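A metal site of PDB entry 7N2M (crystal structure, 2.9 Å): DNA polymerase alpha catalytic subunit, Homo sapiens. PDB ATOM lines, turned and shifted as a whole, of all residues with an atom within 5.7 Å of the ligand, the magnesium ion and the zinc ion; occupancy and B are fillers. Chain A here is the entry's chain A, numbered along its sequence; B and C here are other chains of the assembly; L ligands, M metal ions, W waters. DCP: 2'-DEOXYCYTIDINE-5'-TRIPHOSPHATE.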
ATOM      1  N   ASP A 525     -10.391  15.282  25.714  1.00  0.00           N
ATOM      2  CA  ASP A 525      -9.039  14.778  25.940  1.00  0.00           C
ATOM      3  C   ASP A 525      -8.980  13.939  27.223  1.00  0.00           C
ATOM      4  O   ASP A 525      -9.560  14.323  28.240  1.00  0.00           O
ATOM      5  CB  ASP A 525      -8.032  15.938  26.044  1.00  0.00           C
ATOM      6  CG  ASP A 525      -6.571  15.462  26.185  1.00  0.00           C
ATOM      7  OD1 ASP A 525      -5.938  15.084  25.176  1.00  0.00           O
ATOM      8  OD2 ASP A 525      -6.065  15.455  27.329  1.00  0.00           O
ATOM      9  N   PHE A 526      -8.288  12.813  27.180  1.00  0.00           N
ATOM     10  CA  PHE A 526      -8.137  12.002  28.387  1.00  0.00           C
ATOM     11  C   PHE A 526      -7.189  12.664  29.401  1.00  0.00           C
ATOM     12  O   PHE A 526      -6.184  13.300  29.044  1.00  0.00           O
ATOM     13  CB  PHE A 526      -7.587  10.630  28.057  1.00  0.00           C
ATOM     14  CG  PHE A 526      -8.578   9.719  27.424  1.00  0.00           C
ATOM     15  CD1 PHE A 526      -8.590   9.516  26.054  1.00  0.00           C
ATOM     16  CD2 PHE A 526      -9.490   9.029  28.209  1.00  0.00           C
ATOM     17  CE1 PHE A 526      -9.502   8.640  25.472  1.00  0.00           C
ATOM     18  CE2 PHE A 526     -10.397   8.149  27.635  1.00  0.00           C
ATOM     19  CZ  PHE A 526     -10.399   7.955  26.264  1.00  0.00           C
ATOM     20  N   ASN A 527      -7.532  12.510  30.672  1.00  0.00           N
ATOM     21  CA  ASN A 527      -6.748  13.037  31.782  1.00  0.00           C
ATOM     22  C   ASN A 527      -5.575  12.113  32.064  1.00  0.00           C
ATOM     23  O   ASN A 527      -5.778  10.923  32.347  1.00  0.00           O
ATOM     24  CB  ASN A 527      -7.629  13.167  33.038  1.00  0.00           C
ATOM     25  CG  ASN A 527      -8.552  14.346  32.973  1.00  0.00           C
ATOM     26  OD1 ASN A 527      -8.125  15.469  32.695  1.00  0.00           O
ATOM     27  ND2 ASN A 527      -9.831  14.118  33.238  1.00  0.00           N
ATOM     28  N   SER A 528      -4.355  12.648  31.989  1.00  0.00           N
ATOM     29  CA  SER A 528      -3.148  11.876  32.251  1.00  0.00           C
ATOM     30  C   SER A 528      -3.180  10.462  31.663  1.00  0.00           C
ATOM     31  O   SER A 528      -2.920   9.473  32.353  1.00  0.00           O
ATOM     32  CB  SER A 528      -2.910  11.804  33.766  1.00  0.00           C
ATOM     33  OG  SER A 528      -2.434  13.045  34.259  1.00  0.00           O
ATOM     34  N   LEU A 529      -3.467  10.391  30.367  1.00  0.00           N
ATOM     35  CA  LEU A 529      -3.593   9.123  29.691  1.00  0.00           C
ATOM     36  C   LEU A 529      -2.544   8.064  29.985  1.00  0.00           C
ATOM     37  O   LEU A 529      -2.839   7.068  30.630  1.00  0.00           O
ATOM     38  CB  LEU A 529      -3.689   9.344  28.176  1.00  0.00           C
ATOM     39  CG  LEU A 529      -3.918   8.043  27.411  1.00  0.00           C
ATOM     40  CD1 LEU A 529      -5.241   7.439  27.834  1.00  0.00           C
ATOM     41  CD2 LEU A 529      -3.897   8.298  25.933  1.00  0.00           C
ATOM     42  N   TYR A 530      -1.310   8.255  29.517  1.00  0.00           N
ATOM     43  CA  TYR A 530      -0.302   7.234  29.753  1.00  0.00           C
ATOM     44  C   TYR A 530      -0.145   6.879  31.233  1.00  0.00           C
ATOM     45  O   TYR A 530      -0.080   5.698  31.598  1.00  0.00           O
ATOM     46  CB  TYR A 530       1.020   7.669  29.121  1.00  0.00           C
ATOM     47  CG  TYR A 530       1.074   7.483  27.617  1.00  0.00           C
ATOM     48  CD1 TYR A 530      -0.067   7.659  26.825  1.00  0.00           C
ATOM     49  CD2 TYR A 530       2.271   7.190  26.991  1.00  0.00           C
ATOM     50  CE1 TYR A 530      -0.004   7.549  25.437  1.00  0.00           C
ATOM     51  CE2 TYR A 530       2.348   7.077  25.604  1.00  0.00           C
ATOM     52  CZ  TYR A 530       1.208   7.265  24.834  1.00  0.00           C
ATOM     53  OH  TYR A 530       1.298   7.201  23.457  1.00  0.00           O
ATOM     54  N   PRO A 531      -0.045   7.883  32.128  1.00  0.00           N
ATOM     55  CA  PRO A 531       0.091   7.501  33.535  1.00  0.00           C
ATOM     56  C   PRO A 531      -1.106   6.665  33.993  1.00  0.00           C
ATOM     57  O   PRO A 531      -0.937   5.699  34.748  1.00  0.00           O
ATOM     58  CB  PRO A 531       0.204   8.837  34.238  1.00  0.00           C
ATOM     59  CG  PRO A 531       1.064   9.615  33.255  1.00  0.00           C
ATOM     60  CD  PRO A 531       0.377   9.296  31.936  1.00  0.00           C
ATOM     61  N   ARG A 587      -0.459  16.537  41.033  1.00  0.00           N
ATOM     62  CA  ARG A 587      -0.892  17.412  39.970  1.00  0.00           C
ATOM     63  C   ARG A 587      -2.351  17.825  40.136  1.00  0.00           C
ATOM     64  O   ARG A 587      -2.664  19.013  40.035  1.00  0.00           O
ATOM     65  CB  ARG A 587      -0.686  16.739  38.634  1.00  0.00           C
ATOM     66  CG  ARG A 587      -0.832  17.687  37.471  1.00  0.00           C
ATOM     67  CD  ARG A 587      -0.958  16.921  36.183  1.00  0.00           C
ATOM     68  NE  ARG A 587      -1.423  17.790  35.124  1.00  0.00           N
ATOM     69  CZ  ARG A 587      -1.896  17.337  33.970  1.00  0.00           C
ATOM     70  NH1 ARG A 587      -1.941  16.032  33.743  1.00  0.00           N
ATOM     71  NH2 ARG A 587      -2.318  18.184  33.048  1.00  0.00           N
ATOM     72  N   LYS A 591      -4.177  21.494  40.506  1.00  0.00           N
ATOM     73  CA  LYS A 591      -5.193  21.950  39.576  1.00  0.00           C
ATOM     74  C   LYS A 591      -6.374  22.404  40.396  1.00  0.00           C
ATOM     75  O   LYS A 591      -7.043  23.366  40.047  1.00  0.00           O
ATOM     76  CB  LYS A 591      -5.567  20.838  38.594  1.00  0.00           C
ATOM     77  CG  LYS A 591      -4.375  20.291  37.816  1.00  0.00           C
ATOM     78  CD  LYS A 591      -4.751  19.651  36.509  1.00  0.00           C
ATOM     79  CE  LYS A 591      -5.160  20.706  35.508  1.00  0.00           C
ATOM     80  NZ  LYS A 591      -5.524  20.088  34.221  1.00  0.00           N
ATOM     81  N   GLN A 611       1.813  22.832  37.628  1.00  0.00           N
ATOM     82  CA  GLN A 611       0.948  21.751  37.183  1.00  0.00           C
ATOM     83  C   GLN A 611       1.479  21.017  35.953  1.00  0.00           C
ATOM     84  O   GLN A 611       1.375  19.803  35.870  1.00  0.00           O
ATOM     85  CB  GLN A 611      -0.442  22.314  36.925  1.00  0.00           C
ATOM     86  CG  GLN A 611      -1.394  21.337  36.361  1.00  0.00           C
ATOM     87  CD  GLN A 611      -1.450  21.432  34.872  1.00  0.00           C
ATOM     88  OE1 GLN A 611      -1.869  20.499  34.195  1.00  0.00           O
ATOM     89  NE2 GLN A 611      -1.048  22.586  34.339  1.00  0.00           N
ATOM     90  N   LYS A 615       3.127  17.246  35.278  1.00  0.00           N
ATOM     91  CA  LYS A 615       2.643  16.450  34.152  1.00  0.00           C
ATOM     92  C   LYS A 615       3.866  15.867  33.454  1.00  0.00           C
ATOM     93  O   LYS A 615       3.932  14.668  33.192  1.00  0.00           O
ATOM     94  CB  LYS A 615       1.868  17.344  33.191  1.00  0.00           C
ATOM     95  CG  LYS A 615       1.296  16.647  31.999  1.00  0.00           C
ATOM     96  CD  LYS A 615       0.767  17.694  31.050  1.00  0.00           C
ATOM     97  CE  LYS A 615       0.035  17.111  29.866  1.00  0.00           C
ATOM     98  NZ  LYS A 615      -0.377  18.226  28.977  1.00  0.00           N
ATOM     99  N   LEU A 616       4.835  16.743  33.185  1.00  0.00           N
ATOM    100  CA  LEU A 616       6.078  16.346  32.541  1.00  0.00           C
ATOM    101  C   LEU A 616       6.810  15.257  33.318  1.00  0.00           C
ATOM    102  O   LEU A 616       7.352  14.319  32.739  1.00  0.00           O
ATOM    103  CB  LEU A 616       6.989  17.551  32.394  1.00  0.00           C
ATOM    104  CG  LEU A 616       6.817  18.198  31.021  1.00  0.00           C
ATOM    105  CD1 LEU A 616       7.122  19.693  31.065  1.00  0.00           C
ATOM    106  CD2 LEU A 616       7.715  17.426  30.036  1.00  0.00           C
ATOM    107  N   ASN A 619       5.050  11.980  32.639  1.00  0.00           N
ATOM    108  CA  ASN A 619       5.312  11.467  31.300  1.00  0.00           C
ATOM    109  C   ASN A 619       6.755  11.018  31.122  1.00  0.00           C
ATOM    110  O   ASN A 619       7.031  10.008  30.473  1.00  0.00           O
ATOM    111  CB  ASN A 619       4.920  12.512  30.266  1.00  0.00           C
ATOM    112  CG  ASN A 619       3.417  12.703  30.189  1.00  0.00           C
ATOM    113  OD1 ASN A 619       2.929  13.714  29.703  1.00  0.00           O
ATOM    114  ND2 ASN A 619       2.668  11.717  30.689  1.00  0.00           N
ATOM    115  N   TYR A 622       7.196   7.596  32.039  1.00  0.00           N
ATOM    116  CA  TYR A 622       6.815   6.651  30.978  1.00  0.00           C
ATOM    117  C   TYR A 622       7.970   6.607  29.990  1.00  0.00           C
ATOM    118  O   TYR A 622       8.478   5.535  29.653  1.00  0.00           O
ATOM    119  CB  TYR A 622       5.541   7.131  30.261  1.00  0.00           C
ATOM    120  CG  TYR A 622       5.544   6.874  28.761  1.00  0.00           C
ATOM    121  CD1 TYR A 622       5.443   5.587  28.250  1.00  0.00           C
ATOM    122  CD2 TYR A 622       5.748   7.930  27.856  1.00  0.00           C
ATOM    123  CE1 TYR A 622       5.570   5.346  26.868  1.00  0.00           C
ATOM    124  CE2 TYR A 622       5.872   7.714  26.492  1.00  0.00           C
ATOM    125  CZ  TYR A 622       5.795   6.413  25.997  1.00  0.00           C
ATOM    126  OH  TYR A 622       5.987   6.176  24.642  1.00  0.00           O
ATOM    127  N   ASP A 667      -5.670  13.295  18.271  1.00  0.00           N
ATOM    128  CA  ASP A 667      -4.219  13.167  18.498  1.00  0.00           C
ATOM    129  C   ASP A 667      -3.831  12.444  19.806  1.00  0.00           C
ATOM    130  O   ASP A 667      -3.856  13.035  20.876  1.00  0.00           O
ATOM    131  CB  ASP A 667      -3.579  14.559  18.473  1.00  0.00           C
ATOM    132  CG  ASP A 667      -2.049  14.504  18.427  1.00  0.00           C
ATOM    133  OD1 ASP A 667      -1.465  13.469  18.800  1.00  0.00           O
ATOM    134  OD2 ASP A 667      -1.453  15.521  18.028  1.00  0.00           O
ATOM    135  N   THR A 668      -3.448  11.175  19.691  1.00  0.00           N
ATOM    136  CA  THR A 668      -3.037  10.331  20.818  1.00  0.00           C
ATOM    137  C   THR A 668      -4.105  10.077  21.880  1.00  0.00           C
ATOM    138  O   THR A 668      -4.456   8.931  22.144  1.00  0.00           O
ATOM    139  CB  THR A 668      -1.788  10.904  21.545  1.00  0.00           C
ATOM    140  OG1 THR A 668      -0.776  11.230  20.570  1.00  0.00           O
ATOM    141  CG2 THR A 668      -1.221   9.852  22.533  1.00  0.00           C
ATOM    142  N   ASP A 669      -4.623  11.138  22.496  1.00  0.00           N
ATOM    143  CA  ASP A 669      -5.620  10.995  23.555  1.00  0.00           C
ATOM    144  C   ASP A 669      -6.757  12.000  23.413  1.00  0.00           C
ATOM    145  O   ASP A 669      -7.424  12.329  24.399  1.00  0.00           O
ATOM    146  CB  ASP A 669      -4.983  11.178  24.943  1.00  0.00           C
ATOM    147  CG  ASP A 669      -4.612  12.661  25.253  1.00  0.00           C
ATOM    148  OD1 ASP A 669      -4.729  13.051  26.449  1.00  0.00           O
ATOM    149  OD2 ASP A 669      -4.191  13.424  24.348  1.00  0.00           O
ATOM    150  N   SER A 670      -6.977  12.508  22.205  1.00  0.00           N
ATOM    151  CA  SER A 670      -8.050  13.479  22.010  1.00  0.00           C
ATOM    152  C   SER A 670      -8.952  13.149  20.836  1.00  0.00           C
ATOM    153  O   SER A 670      -8.611  12.339  19.983  1.00  0.00           O
ATOM    154  CB  SER A 670      -7.482  14.891  21.840  1.00  0.00           C
ATOM    155  OG  SER A 670      -6.544  14.983  20.775  1.00  0.00           O
ATOM    156  N   ASP A 706     -11.939  19.193  26.928  1.00  0.00           N
ATOM    157  CA  ASP A 706     -10.765  20.068  26.975  1.00  0.00           C
ATOM    158  C   ASP A 706     -11.093  21.469  26.455  1.00  0.00           C
ATOM    159  O   ASP A 706     -10.457  22.459  26.848  1.00  0.00           O
ATOM    160  CB  ASP A 706      -9.617  19.463  26.175  1.00  0.00           C
ATOM    161  CG  ASP A 706      -8.255  19.956  26.643  1.00  0.00           C
ATOM    162  OD1 ASP A 706      -7.833  19.584  27.756  1.00  0.00           O
ATOM    163  OD2 ASP A 706      -7.614  20.727  25.893  1.00  0.00           O
ATOM    164  P    DG B   4      16.963  13.802  29.698  1.00  0.00           P
ATOM    165  OP1  DG B   4      15.989  14.868  29.356  1.00  0.00           O
ATOM    166  OP2  DG B   4      17.510  13.712  31.080  1.00  0.00           O
ATOM    167  O5'  DG B   4      16.334  12.380  29.388  1.00  0.00           O
ATOM    168  C5'  DG B   4      15.711  12.137  28.159  1.00  0.00           C
ATOM    169  C4'  DG B   4      14.703  11.027  28.299  1.00  0.00           C
ATOM    170  O4'  DG B   4      13.693  11.435  29.246  1.00  0.00           O
ATOM    171  C3'  DG B   4      13.947  10.746  27.027  1.00  0.00           C
ATOM    172  O3'  DG B   4      14.523   9.656  26.350  1.00  0.00           O
ATOM    173  C2'  DG B   4      12.596  10.275  27.516  1.00  0.00           C
ATOM    174  C1'  DG B   4      12.398  11.009  28.818  1.00  0.00           C
ATOM    175  N9   DG B   4      11.643  12.225  28.574  1.00  0.00           N
ATOM    176  C8   DG B   4      12.106  13.506  28.740  1.00  0.00           C
ATOM    177  N7   DG B   4      11.223  14.412  28.423  1.00  0.00           N
ATOM    178  C5   DG B   4      10.117  13.687  28.024  1.00  0.00           C
ATOM    179  C6   DG B   4       8.846  14.139  27.565  1.00  0.00           C
ATOM    180  O6   DG B   4       8.447  15.303  27.440  1.00  0.00           O
ATOM    181  N1   DG B   4       8.015  13.078  27.249  1.00  0.00           N
ATOM    182  C2   DG B   4       8.345  11.755  27.359  1.00  0.00           C
ATOM    183  N2   DG B   4       7.417  10.869  26.991  1.00  0.00           N
ATOM    184  N3   DG B   4       9.520  11.323  27.801  1.00  0.00           N
ATOM    185  C4   DG B   4      10.353  12.339  28.114  1.00  0.00           C
ATOM    186  P    DT B   5      14.377   9.587  24.774  1.00  0.00           P
ATOM    187  OP1  DT B   5      15.327   8.565  24.240  1.00  0.00           O
ATOM    188  OP2  DT B   5      14.458  10.999  24.334  1.00  0.00           O
ATOM    189  O5'  DT B   5      12.885   9.097  24.568  1.00  0.00           O
ATOM    190  C5'  DT B   5      12.492   7.807  25.003  1.00  0.00           C
ATOM    191  C4'  DT B   5      11.103   7.496  24.481  1.00  0.00           C
ATOM    192  O4'  DT B   5      10.171   8.385  25.136  1.00  0.00           O
ATOM    193  C3'  DT B   5      10.938   7.774  22.997  1.00  0.00           C
ATOM    194  O3'  DT B   5      11.042   6.552  22.259  1.00  0.00           O
ATOM    195  C2'  DT B   5       9.478   8.167  22.884  1.00  0.00           C
ATOM    196  C1'  DT B   5       9.119   8.737  24.246  1.00  0.00           C
ATOM    197  N1   DT B   5       9.010  10.196  24.238  1.00  0.00           N
ATOM    198  C2   DT B   5       7.788  10.744  23.977  1.00  0.00           C
ATOM    199  O2   DT B   5       6.791  10.068  23.770  1.00  0.00           O
ATOM    200  N3   DT B   5       7.775  12.115  23.939  1.00  0.00           N
ATOM    201  C4   DT B   5       8.852  12.956  24.144  1.00  0.00           C
ATOM    202  O4   DT B   5       8.702  14.180  24.077  1.00  0.00           O
ATOM    203  C5   DT B   5      10.092  12.308  24.437  1.00  0.00           C
ATOM    204  C7   DT B   5      11.312  13.144  24.677  1.00  0.00           C
ATOM    205  C6   DT B   5      10.116  10.978  24.480  1.00  0.00           C
ATOM    206  P     C C  11      -0.371  19.304  21.538  1.00  0.00           P
ATOM    207  OP1   C C  11      -1.835  19.604  21.590  1.00  0.00           O
ATOM    208  OP2   C C  11       0.588  20.130  22.332  1.00  0.00           O
ATOM    209  O5'   C C  11      -0.094  17.760  21.886  1.00  0.00           O
ATOM    210  C5'   C C  11      -1.013  16.772  21.444  1.00  0.00           C
ATOM    211  C4'   C C  11      -0.391  15.398  21.425  1.00  0.00           C
ATOM    212  O4'   C C  11       0.983  15.462  21.009  1.00  0.00           O
ATOM    213  C3'   C C  11      -0.326  14.742  22.797  1.00  0.00           C
ATOM    214  C2'   C C  11       0.850  13.780  22.674  1.00  0.00           C
ATOM    215  C1'   C C  11       1.736  14.429  21.642  1.00  0.00           C
ATOM    216  N1    C C  11       2.951  15.021  22.210  1.00  0.00           N
ATOM    217  C2    C C  11       3.969  14.177  22.613  1.00  0.00           C
ATOM    218  O2    C C  11       3.802  12.954  22.486  1.00  0.00           O
ATOM    219  N3    C C  11       5.112  14.707  23.135  1.00  0.00           N
ATOM    220  C4    C C  11       5.227  16.030  23.268  1.00  0.00           C
ATOM    221  N4    C C  11       6.350  16.519  23.791  1.00  0.00           N
ATOM    222  C5    C C  11       4.192  16.914  22.862  1.00  0.00           C
ATOM    223  C6    C C  11       3.076  16.376  22.344  1.00  0.00           C
HETATM  224  N1  DCP L   1       2.983  12.553  26.192  1.00  0.00           N
HETATM  225  C2  DCP L   1       4.335  12.338  26.458  1.00  0.00           C
HETATM  226  N3  DCP L   1       5.178  13.382  26.643  1.00  0.00           N
HETATM  227  C4  DCP L   1       4.732  14.657  26.570  1.00  0.00           C
HETATM  228  C5  DCP L   1       3.344  14.921  26.292  1.00  0.00           C
HETATM  229  C6  DCP L   1       2.501  13.858  26.122  1.00  0.00           C
HETATM  230  O2  DCP L   1       4.779  11.202  26.529  1.00  0.00           O
HETATM  231  N4  DCP L   1       5.598  15.707  26.755  1.00  0.00           N
HETATM  232  C1' DCP L   1       2.062  11.394  26.000  1.00  0.00           C
HETATM  233  C2' DCP L   1       1.660  10.859  27.352  1.00  0.00           C
HETATM  234  C3' DCP L   1       0.330  11.541  27.606  1.00  0.00           C
HETATM  235  C4' DCP L   1      -0.307  11.494  26.197  1.00  0.00           C
HETATM  236  O4' DCP L   1       0.834  11.774  25.323  1.00  0.00           O
HETATM  237  O3' DCP L   1      -0.433  10.766  28.536  1.00  0.00           O
HETATM  238  C5' DCP L   1      -1.379  12.610  25.986  1.00  0.00           C
HETATM  239  O5' DCP L   1      -0.743  13.875  25.920  1.00  0.00           O
HETATM  240  PA  DCP L   1      -1.466  14.996  26.834  1.00  0.00           P
HETATM  241  O1A DCP L   1      -2.942  14.947  26.674  1.00  0.00           O
HETATM  242  O2A DCP L   1      -0.916  16.462  26.405  1.00  0.00           O
HETATM  243  O3A DCP L   1      -0.961  14.671  28.339  1.00  0.00           O
HETATM  244  PB  DCP L   1      -1.986  13.940  29.331  1.00  0.00           P
HETATM  245  O1B DCP L   1      -3.349  13.460  28.607  1.00  0.00           O
HETATM  246  O2B DCP L   1      -1.352  12.770  29.928  1.00  0.00           O
HETATM  247  O3B DCP L   1      -2.227  15.070  30.454  1.00  0.00           O
HETATM  248  PG  DCP L   1      -3.544  15.924  30.310  1.00  0.00           P
HETATM  249  O1G DCP L   1      -4.557  15.451  31.466  1.00  0.00           O
HETATM  250  O2G DCP L   1      -3.186  17.342  30.461  1.00  0.00           O
HETATM  251  O3G DCP L   1      -4.241  15.720  28.880  1.00  0.00           O
HETATM  252 MG    MG M   1      -4.952  14.136  27.906  1.00  0.00          MG
HETATM  253 ZN    ZN M   2      -3.978  15.485  24.584  1.00  0.00          ZN
HETATM  254  O   HOH W   1       4.003  18.041  26.529  1.00  0.00           O
HETATM  255  O   HOH W   2       0.663  12.957  32.297  1.00  0.00           O
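The backbone NH (N) of Ser 528 lies within hydrogen-bond range of an oxygen (O1G) of the ligand. The side-chain amino group (NZ) of Lys 615 is in salt-bridge range of an oxygen (O2A) of the ligand (3.2 Å). N4 of C 11 of chain C sits at hydrogen-bond distance from a nitrogen (N4) of the ligand (3.2 Å). An oxygen (O2G) of the ligand is in salt-bridge range of the guanidinium group (NH2) of Arg 587. N4 of the ligand lies within hydrogen-bond range of O6 of DG 4 of chain B (3.0 Å). N of Tyr 530 lies within hydrogen-bond range of O3' of the ligand, at 2.8 Å. The backbone NH of Leu 529 sits at hydrogen-bond distance from an oxygen (O2B) of the ligand (3.2 Å).
NH1 of Arg 587 sits at hydrogen-bond distance from OG of Ser 528, 3.1 Å away. The side-chain hydroxyl of Thr 668 lies within hydrogen-bond range of the side-chain carboxylate of Asp 667 (2.9 Å). The side-chain amide oxygen (OE1) of Gln 611 is in hydrogen-bond range of the guanidinium group (NH2) of Arg 587.
Asn 527 touches the ligand (CA to O1G, 3.3 Å). Pro 531 touches the ligand. Asn 619 touches the ligand. CE2 of Tyr 622 touches O2 of the ligand, at 3.7 Å. Thr 668 touches the ligand. DT 5 of chain B touches the ligand (O2 to O2, 3.6 Å). Hydrophobic or aromatic side chains within 4 Å of the ligand: Leu 529, Tyr 530, Pro 531 and Tyr 622. Of the 22 residues printed, 16 come within 4 Å of the ligand. The nearest printed residue that does not touch the ligand is Leu 616 (4.3 Å).
Within 4 Å of the magnesium ion: Asp 525, Phe 526 and Asp 669. The nearest printed residue that does not touch the magnesium ion is Asn 527 (4.1 Å).
Within 4 Å of the zinc ion: Asp 525 and Asp 669.
The magnesium ion is bound by the side-chain carboxylate (OD2) of Asp 525 (1.8 Å), the side-chain carboxylate (OD1) of Asp 669 (1.8 Å), the backbone carbonyl oxygen (O) of Phe 526 (1.9 Å), an oxygen (O1B) of the ligand (1.9 Å), an oxygen (O3G) of the ligand (2.0 Å) and an oxygen (O1A) of the ligand (2.5 Å).
The zinc ion is bound by the side-chain carboxylate (OD2) of Asp 669 (2.1 Å), the side-chain carboxylate (OD1) of Asp 525 (2.1 Å) and an oxygen (O1A) of the ligand (2.4 Å).
Water W2 bridges ND2 of Asn 619 and O2B of the ligand.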
